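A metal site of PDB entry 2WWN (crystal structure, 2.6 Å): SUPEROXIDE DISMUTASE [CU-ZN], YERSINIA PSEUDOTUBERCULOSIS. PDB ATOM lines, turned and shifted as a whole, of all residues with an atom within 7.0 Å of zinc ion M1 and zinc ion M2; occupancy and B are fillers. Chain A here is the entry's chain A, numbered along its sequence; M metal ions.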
ATOM      1  N   GLY A  60      -1.965 -21.852  11.633  1.00  0.00           N
ATOM      2  CA  GLY A  60      -2.191 -20.557  11.033  1.00  0.00           C
ATOM      3  C   GLY A  60      -1.613 -20.550   9.631  1.00  0.00           C
ATOM      4  O   GLY A  60      -0.492 -21.027   9.401  1.00  0.00           O
ATOM      5  N   PHE A  61      -2.370 -19.993   8.685  1.00  0.00           N
ATOM      6  CA  PHE A  61      -2.031 -20.094   7.275  1.00  0.00           C
ATOM      7  C   PHE A  61      -2.410 -18.786   6.596  1.00  0.00           C
ATOM      8  O   PHE A  61      -3.566 -18.591   6.213  1.00  0.00           O
ATOM      9  CB  PHE A  61      -2.803 -21.273   6.670  1.00  0.00           C
ATOM     10  CG  PHE A  61      -2.311 -21.704   5.307  1.00  0.00           C
ATOM     11  CD1 PHE A  61      -0.956 -21.737   5.016  1.00  0.00           C
ATOM     12  CD2 PHE A  61      -3.221 -22.118   4.330  1.00  0.00           C
ATOM     13  CE1 PHE A  61      -0.507 -22.152   3.781  1.00  0.00           C
ATOM     14  CE2 PHE A  61      -2.782 -22.534   3.095  1.00  0.00           C
ATOM     15  CZ  PHE A  61      -1.427 -22.554   2.811  1.00  0.00           C
ATOM     16  N   HIS A  62      -1.449 -17.878   6.460  1.00  0.00           N
ATOM     17  CA  HIS A  62      -1.758 -16.525   6.000  1.00  0.00           C
ATOM     18  C   HIS A  62      -0.828 -16.051   4.876  1.00  0.00           C
ATOM     19  O   HIS A  62       0.262 -16.577   4.698  1.00  0.00           O
ATOM     20  CB  HIS A  62      -1.676 -15.535   7.170  1.00  0.00           C
ATOM     21  CG  HIS A  62      -2.098 -16.123   8.489  1.00  0.00           C
ATOM     22  ND1 HIS A  62      -1.212 -16.312   9.530  1.00  0.00           N
ATOM     23  CD2 HIS A  62      -3.299 -16.554   8.933  1.00  0.00           C
ATOM     24  CE1 HIS A  62      -1.860 -16.833  10.559  1.00  0.00           C
ATOM     25  NE2 HIS A  62      -3.125 -16.992  10.222  1.00  0.00           N
ATOM     26  N   LEU A  63      -1.284 -15.046   4.126  1.00  0.00           N
ATOM     27  CA  LEU A  63      -0.432 -14.358   3.164  1.00  0.00           C
ATOM     28  C   LEU A  63       0.162 -13.127   3.817  1.00  0.00           C
ATOM     29  O   LEU A  63      -0.560 -12.314   4.395  1.00  0.00           O
ATOM     30  CB  LEU A  63      -1.224 -13.938   1.929  1.00  0.00           C
ATOM     31  CG  LEU A  63      -1.702 -15.046   0.997  1.00  0.00           C
ATOM     32  CD1 LEU A  63      -2.751 -14.504   0.052  1.00  0.00           C
ATOM     33  CD2 LEU A  63      -0.530 -15.657   0.232  1.00  0.00           C
ATOM     34  N   HIS A  64       1.480 -12.990   3.741  1.00  0.00           N
ATOM     35  CA  HIS A  64       2.147 -11.831   4.313  1.00  0.00           C
ATOM     36  C   HIS A  64       2.541 -10.839   3.214  1.00  0.00           C
ATOM     37  O   HIS A  64       2.653 -11.213   2.039  1.00  0.00           O
ATOM     38  CB  HIS A  64       3.339 -12.264   5.162  1.00  0.00           C
ATOM     39  CG  HIS A  64       2.946 -12.923   6.448  1.00  0.00           C
ATOM     40  ND1 HIS A  64       3.437 -12.511   7.670  1.00  0.00           N
ATOM     41  CD2 HIS A  64       2.089 -13.942   6.702  1.00  0.00           C
ATOM     42  CE1 HIS A  64       2.909 -13.267   8.624  1.00  0.00           C
ATOM     43  NE2 HIS A  64       2.090 -14.141   8.062  1.00  0.00           N
ATOM     44  N   GLY A  85       7.146  -9.425   6.580  1.00  0.00           N
ATOM     45  CA  GLY A  85       6.257  -8.406   7.122  1.00  0.00           C
ATOM     46  C   GLY A  85       5.033  -9.015   7.777  1.00  0.00           C
ATOM     47  O   GLY A  85       5.004 -10.219   8.040  1.00  0.00           O
ATOM     48  N   GLY A  86       4.035  -8.185   8.056  1.00  0.00           N
ATOM     49  CA  GLY A  86       2.809  -8.647   8.673  1.00  0.00           C
ATOM     50  C   GLY A  86       1.873  -9.265   7.660  1.00  0.00           C
ATOM     51  O   GLY A  86       2.292  -9.585   6.534  1.00  0.00           O
ATOM     52  N   HIS A  87       0.609  -9.428   8.035  1.00  0.00           N
ATOM     53  CA  HIS A  87      -0.395  -9.987   7.128  1.00  0.00           C
ATOM     54  C   HIS A  87      -0.818  -9.014   6.035  1.00  0.00           C
ATOM     55  O   HIS A  87      -0.931  -7.803   6.265  1.00  0.00           O
ATOM     56  CB  HIS A  87      -1.628 -10.474   7.903  1.00  0.00           C
ATOM     57  CG  HIS A  87      -1.352 -11.606   8.835  1.00  0.00           C
ATOM     58  ND1 HIS A  87      -2.121 -11.846   9.956  1.00  0.00           N
ATOM     59  CD2 HIS A  87      -0.400 -12.565   8.827  1.00  0.00           C
ATOM     60  CE1 HIS A  87      -1.649 -12.896  10.592  1.00  0.00           C
ATOM     61  NE2 HIS A  87      -0.610 -13.359   9.933  1.00  0.00           N
ATOM     62  N   LEU A  88      -1.057  -9.555   4.833  1.00  0.00           N
ATOM     63  CA  LEU A  88      -1.565  -8.788   3.712  1.00  0.00           C
ATOM     64  C   LEU A  88      -2.856  -8.064   4.105  1.00  0.00           C
ATOM     65  O   LEU A  88      -3.849  -8.706   4.455  1.00  0.00           O
ATOM     66  CB  LEU A  88      -1.805  -9.716   2.521  1.00  0.00           C
ATOM     67  CG  LEU A  88      -2.303  -9.127   1.203  1.00  0.00           C
ATOM     68  CD1 LEU A  88      -1.291  -8.151   0.603  1.00  0.00           C
ATOM     69  CD2 LEU A  88      -2.615 -10.256   0.225  1.00  0.00           C
ATOM     70  N   VAL A  95      -6.505  -5.578  11.539  1.00  0.00           N
ATOM     71  CA  VAL A  95      -7.134  -6.568  12.413  1.00  0.00           C
ATOM     72  C   VAL A  95      -7.182  -7.962  11.786  1.00  0.00           C
ATOM     73  O   VAL A  95      -7.309  -8.109  10.567  1.00  0.00           O
ATOM     74  CB  VAL A  95      -8.548  -6.103  12.855  1.00  0.00           C
ATOM     75  CG1 VAL A  95      -9.505  -6.134  11.672  1.00  0.00           C
ATOM     76  CG2 VAL A  95      -9.054  -6.955  13.996  1.00  0.00           C
ATOM     77  N   HIS A  96      -7.075  -8.990  12.631  1.00  0.00           N
ATOM     78  CA  HIS A  96      -7.098 -10.382  12.170  1.00  0.00           C
ATOM     79  C   HIS A  96      -8.482 -11.011  12.406  1.00  0.00           C
ATOM     80  O   HIS A  96      -8.894 -11.229  13.560  1.00  0.00           O
ATOM     81  CB  HIS A  96      -6.001 -11.175  12.874  1.00  0.00           C
ATOM     82  CG  HIS A  96      -5.887 -12.608  12.441  1.00  0.00           C
ATOM     83  ND1 HIS A  96      -5.078 -13.013  11.399  1.00  0.00           N
ATOM     84  CD2 HIS A  96      -6.476 -13.731  12.918  1.00  0.00           C
ATOM     85  CE1 HIS A  96      -5.181 -14.323  11.250  1.00  0.00           C
ATOM     86  NE2 HIS A  96      -6.022 -14.785  12.157  1.00  0.00           N
ATOM     87  N   LEU A  97      -9.201 -11.296  11.319  1.00  0.00           N
ATOM     88  CA  LEU A  97     -10.578 -11.784  11.434  1.00  0.00           C
ATOM     89  C   LEU A  97     -10.901 -13.007  10.563  1.00  0.00           C
ATOM     90  O   LEU A  97     -12.056 -13.433  10.481  1.00  0.00           O
ATOM     91  CB  LEU A  97     -11.585 -10.660  11.182  1.00  0.00           C
ATOM     92  CG  LEU A  97     -11.679  -9.639  12.332  1.00  0.00           C
ATOM     93  CD1 LEU A  97     -12.497  -8.414  11.948  1.00  0.00           C
ATOM     94  CD2 LEU A  97     -12.238 -10.314  13.581  1.00  0.00           C
ATOM     95  N   GLY A  98      -9.895 -13.585   9.915  1.00  0.00           N
ATOM     96  CA  GLY A  98     -10.073 -14.829   9.202  1.00  0.00           C
ATOM     97  C   GLY A  98     -10.538 -14.708   7.758  1.00  0.00           C
ATOM     98  O   GLY A  98     -10.760 -13.614   7.256  1.00  0.00           O
ATOM     99  N   GLY A 104     -11.319  -7.831   8.211  1.00  0.00           N
ATOM    100  CA  GLY A 104      -9.964  -8.116   8.619  1.00  0.00           C
ATOM    101  C   GLY A 104      -8.992  -8.250   7.457  1.00  0.00           C
ATOM    102  O   GLY A 104      -9.340  -7.973   6.307  1.00  0.00           O
ATOM    103  N   HIS A 105      -7.773  -8.679   7.781  1.00  0.00           N
ATOM    104  CA  HIS A 105      -6.701  -8.861   6.802  1.00  0.00           C
ATOM    105  C   HIS A 105      -7.118  -9.713   5.599  1.00  0.00           C
ATOM    106  O   HIS A 105      -7.481 -10.883   5.734  1.00  0.00           O
ATOM    107  CB  HIS A 105      -5.494  -9.541   7.466  1.00  0.00           C
ATOM    108  CG  HIS A 105      -4.918  -8.786   8.617  1.00  0.00           C
ATOM    109  ND1 HIS A 105      -4.444  -9.402   9.757  1.00  0.00           N
ATOM    110  CD2 HIS A 105      -4.719  -7.456   8.800  1.00  0.00           C
ATOM    111  CE1 HIS A 105      -3.991  -8.493  10.597  1.00  0.00           C
ATOM    112  NE2 HIS A 105      -4.144  -7.303  10.044  1.00  0.00           N
ATOM    113  N   LEU A 106      -7.013  -9.138   4.398  1.00  0.00           N
ATOM    114  CA  LEU A 106      -7.286  -9.889   3.174  1.00  0.00           C
ATOM    115  C   LEU A 106      -6.423 -11.157   3.079  1.00  0.00           C
ATOM    116  O   LEU A 106      -6.815 -12.135   2.433  1.00  0.00           O
ATOM    117  CB  LEU A 106      -7.046  -9.028   1.937  1.00  0.00           C
ATOM    118  CG  LEU A 106      -7.249  -9.730   0.582  1.00  0.00           C
ATOM    119  CD1 LEU A 106      -8.691 -10.170   0.403  1.00  0.00           C
ATOM    120  CD2 LEU A 106      -6.818  -8.837  -0.573  1.00  0.00           C
ATOM    121  N   GLY A 107      -5.261 -11.133   3.718  1.00  0.00           N
ATOM    122  CA  GLY A 107      -4.329 -12.248   3.658  1.00  0.00           C
ATOM    123  C   GLY A 107      -4.684 -13.416   4.555  1.00  0.00           C
ATOM    124  O   GLY A 107      -3.895 -14.358   4.680  1.00  0.00           O
ATOM    125  N   ASP A 108      -5.850 -13.363   5.186  1.00  0.00           N
ATOM    126  CA  ASP A 108      -6.288 -14.406   6.105  1.00  0.00           C
ATOM    127  C   ASP A 108      -6.894 -15.608   5.381  1.00  0.00           C
ATOM    128  O   ASP A 108      -7.958 -15.501   4.761  1.00  0.00           O
ATOM    129  CB  ASP A 108      -7.302 -13.864   7.107  1.00  0.00           C
ATOM    130  CG  ASP A 108      -6.658 -12.971   8.141  1.00  0.00           C
ATOM    131  OD1 ASP A 108      -5.420 -12.803   8.086  1.00  0.00           O
ATOM    132  OD2 ASP A 108      -7.374 -12.449   9.026  1.00  0.00           O
ATOM    133  N   LEU A 109      -6.211 -16.748   5.478  1.00  0.00           N
ATOM    134  CA  LEU A 109      -6.712 -17.984   4.910  1.00  0.00           C
ATOM    135  C   LEU A 109      -7.220 -18.900   6.020  1.00  0.00           C
ATOM    136  O   LEU A 109      -6.961 -18.649   7.198  1.00  0.00           O
ATOM    137  CB  LEU A 109      -5.616 -18.662   4.091  1.00  0.00           C
ATOM    138  CG  LEU A 109      -4.794 -17.720   3.209  1.00  0.00           C
ATOM    139  CD1 LEU A 109      -3.655 -18.457   2.521  1.00  0.00           C
ATOM    140  CD2 LEU A 109      -5.678 -16.993   2.202  1.00  0.00           C
ATOM    141  N   MET A 141       2.558 -18.192   4.331  1.00  0.00           N
ATOM    142  CA  MET A 141       3.180 -18.462   5.624  1.00  0.00           C
ATOM    143  C   MET A 141       2.493 -19.580   6.409  1.00  0.00           C
ATOM    144  O   MET A 141       1.265 -19.691   6.412  1.00  0.00           O
ATOM    145  CB  MET A 141       3.194 -17.189   6.475  1.00  0.00           C
ATOM    146  CG  MET A 141       4.126 -17.251   7.670  1.00  0.00           C
ATOM    147  SD  MET A 141       5.861 -17.003   7.228  1.00  0.00           S
ATOM    148  CE  MET A 141       5.800 -15.315   6.626  1.00  0.00           C
ATOM    149  N   ILE A 142       3.305 -20.395   7.093  1.00  0.00           N
ATOM    150  CA  ILE A 142       2.797 -21.481   7.930  1.00  0.00           C
ATOM    151  C   ILE A 142       3.329 -21.358   9.359  1.00  0.00           C
ATOM    152  O   ILE A 142       4.534 -21.346   9.583  1.00  0.00           O
ATOM    153  CB  ILE A 142       3.161 -22.864   7.353  1.00  0.00           C
ATOM    154  CG1 ILE A 142       2.610 -23.007   5.933  1.00  0.00           C
ATOM    155  CG2 ILE A 142       2.621 -23.965   8.251  1.00  0.00           C
ATOM    156  CD1 ILE A 142       2.976 -24.294   5.260  1.00  0.00           C
ATOM    157  N   HIS A 143       2.410 -21.263  10.316  1.00  0.00           N
ATOM    158  CA  HIS A 143       2.780 -20.998  11.708  1.00  0.00           C
ATOM    159  C   HIS A 143       2.887 -22.256  12.555  1.00  0.00           C
ATOM    160  O   HIS A 143       2.453 -23.340  12.151  1.00  0.00           O
ATOM    161  CB  HIS A 143       1.796 -20.019  12.350  1.00  0.00           C
ATOM    162  CG  HIS A 143       1.911 -18.628  11.823  1.00  0.00           C
ATOM    163  ND1 HIS A 143       2.739 -17.674  12.400  1.00  0.00           N
ATOM    164  CD2 HIS A 143       1.308 -18.015  10.776  1.00  0.00           C
ATOM    165  CE1 HIS A 143       2.632 -16.538  11.731  1.00  0.00           C
ATOM    166  NE2 HIS A 143       1.771 -16.719  10.745  1.00  0.00           N
ATOM    167  N   ASP A 147      -5.111 -21.131  14.398  1.00  0.00           N
ATOM    168  CA  ASP A 147      -5.774 -19.880  14.049  1.00  0.00           C
ATOM    169  C   ASP A 147      -7.260 -19.917  14.390  1.00  0.00           C
ATOM    170  O   ASP A 147      -8.011 -20.719  13.838  1.00  0.00           O
ATOM    171  CB  ASP A 147      -5.597 -19.548  12.559  1.00  0.00           C
ATOM    172  CG  ASP A 147      -5.983 -18.108  12.229  1.00  0.00           C
ATOM    173  OD1 ASP A 147      -6.553 -17.434  13.120  1.00  0.00           O
ATOM    174  OD2 ASP A 147      -5.720 -17.666  11.095  1.00  0.00           O
ATOM    175  N   ASP A 151      -8.183 -11.724  17.100  1.00  0.00           N
ATOM    176  CA  ASP A 151      -7.055 -11.200  17.865  1.00  0.00           C
ATOM    177  C   ASP A 151      -7.161 -11.561  19.344  1.00  0.00           C
ATOM    178  O   ASP A 151      -6.284 -11.218  20.137  1.00  0.00           O
ATOM    179  CB  ASP A 151      -6.938  -9.680  17.678  1.00  0.00           C
ATOM    180  CG  ASP A 151      -6.457  -9.288  16.288  1.00  0.00           C
ATOM    181  OD1 ASP A 151      -5.582  -9.990  15.750  1.00  0.00           O
ATOM    182  OD2 ASP A 151      -6.956  -8.277  15.733  1.00  0.00           O
ATOM    183  N   LEU A 156      -3.330 -12.215  16.162  1.00  0.00           N
ATOM    184  CA  LEU A 156      -3.177 -12.912  14.887  1.00  0.00           C
ATOM    185  C   LEU A 156      -3.555 -14.385  14.965  1.00  0.00           C
ATOM    186  O   LEU A 156      -2.868 -15.238  14.406  1.00  0.00           O
ATOM    187  CB  LEU A 156      -1.751 -12.755  14.377  1.00  0.00           C
ATOM    188  CG  LEU A 156      -1.300 -11.293  14.241  1.00  0.00           C
ATOM    189  CD1 LEU A 156       0.191 -11.197  13.954  1.00  0.00           C
ATOM    190  CD2 LEU A 156      -2.112 -10.579  13.176  1.00  0.00           C
ATOM    191  N   GLY A 157      -4.654 -14.682  15.671  1.00  0.00           N
ATOM    192  CA  GLY A 157      -5.203 -16.023  15.717  1.00  0.00           C
ATOM    193  C   GLY A 157      -4.423 -17.015  16.548  1.00  0.00           C
ATOM    194  O   GLY A 157      -4.807 -18.179  16.674  1.00  0.00           O
ATOM    195  N   GLY A 159      -1.227 -17.742  15.901  1.00  0.00           N
ATOM    196  CA  GLY A 159      -0.291 -18.400  15.022  1.00  0.00           C
ATOM    197  C   GLY A 159       1.096 -18.512  15.634  1.00  0.00           C
ATOM    198  O   GLY A 159       1.760 -19.548  15.498  1.00  0.00           O
ATOM    199  N   GLY A 160       1.529 -17.456  16.312  1.00  0.00           N
ATOM    200  CA  GLY A 160       2.840 -17.425  16.930  1.00  0.00           C
ATOM    201  C   GLY A 160       3.962 -17.488  15.915  1.00  0.00           C
ATOM    202  O   GLY A 160       3.915 -16.832  14.878  1.00  0.00           O
ATOM    203  N   ARG A 162       6.751 -18.286  13.042  1.00  0.00           N
ATOM    204  CA  ARG A 162       6.679 -18.665  11.638  1.00  0.00           C
ATOM    205  C   ARG A 162       7.583 -19.871  11.431  1.00  0.00           C
ATOM    206  O   ARG A 162       8.766 -19.817  11.728  1.00  0.00           O
ATOM    207  CB  ARG A 162       7.115 -17.487  10.748  1.00  0.00           C
ATOM    208  CG  ARG A 162       6.457 -16.184  11.156  1.00  0.00           C
ATOM    209  CD  ARG A 162       6.791 -15.007  10.258  1.00  0.00           C
ATOM    210  NE  ARG A 162       6.139 -13.784  10.745  1.00  0.00           N
ATOM    211  CZ  ARG A 162       6.137 -12.615  10.116  1.00  0.00           C
ATOM    212  NH1 ARG A 162       6.742 -12.480   8.944  1.00  0.00           N
ATOM    213  NH2 ARG A 162       5.512 -11.582  10.662  1.00  0.00           N
HETATM  214 ZN    ZN M   1       0.768 -15.057   9.700  1.00  0.00          ZN
HETATM  215 ZN    ZN M   2      -4.426 -11.755   9.639  1.00  0.00          ZN
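Within 4 Å of zinc ion M2: His 87, His 96, His 105 and Asp 108. The nearest printed residue that does not touch zinc ion M2 is Leu 156 (4.4 Å).
Of the 29 residues printed, 4 come within 4 Å of zinc ion M1.
Zinc ion M2 is bound by OD1 of Asp 108 (2.1 Å), ND1 of His 96 (2.3 Å), ND1 of His 87 (2.3 Å) and ND1 of His 105 (2.4 Å). Zinc ion M2 has four donor atoms within binding distance.
N of Leu 97 sits at hydrogen-bond distance from OD2 of Asp 108 (3.2 Å). A ring nitrogen (ND1) of His 143 lies within hydrogen-bond range of the backbone carbonyl oxygen of Gly 160 (2.9 Å). OD2 of Asp 151 lies within hydrogen-bond range of N of His 96 (3.2 Å). A ring nitrogen (ND1) of His 64 sits close to the backbone carbonyl oxygen (O) of Gly 86 (3.3 Å). ND1 of His 64 is in hydrogen-bond range of O of Gly 85, at 2.8 Å. The backbone carbonyl oxygen of His 62 is in hydrogen-bond range of the backbone NH of Met 141 (2.8 Å). A ring nitrogen (NE2) of His 62 lies within hydrogen-bond range of the side-chain carboxylate (OD2) of Asp 147, at 2.8 Å. The backbone NH (N) of His 105 lies within hydrogen-bond range of the backbone carbonyl oxygen (O) of Val 95, 2.9 Å away.
Zinc ion M1 is bound by a ring nitrogen (NE2) of His 87 (2.2 Å), a ring nitrogen (NE2) of His 143 (2.2 Å), a ring nitrogen (NE2) of His 64 (2.3 Å) and a ring nitrogen (ND1) of His 62 (2.4 Å). Zinc ion M1 has four donor atoms within binding distance.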
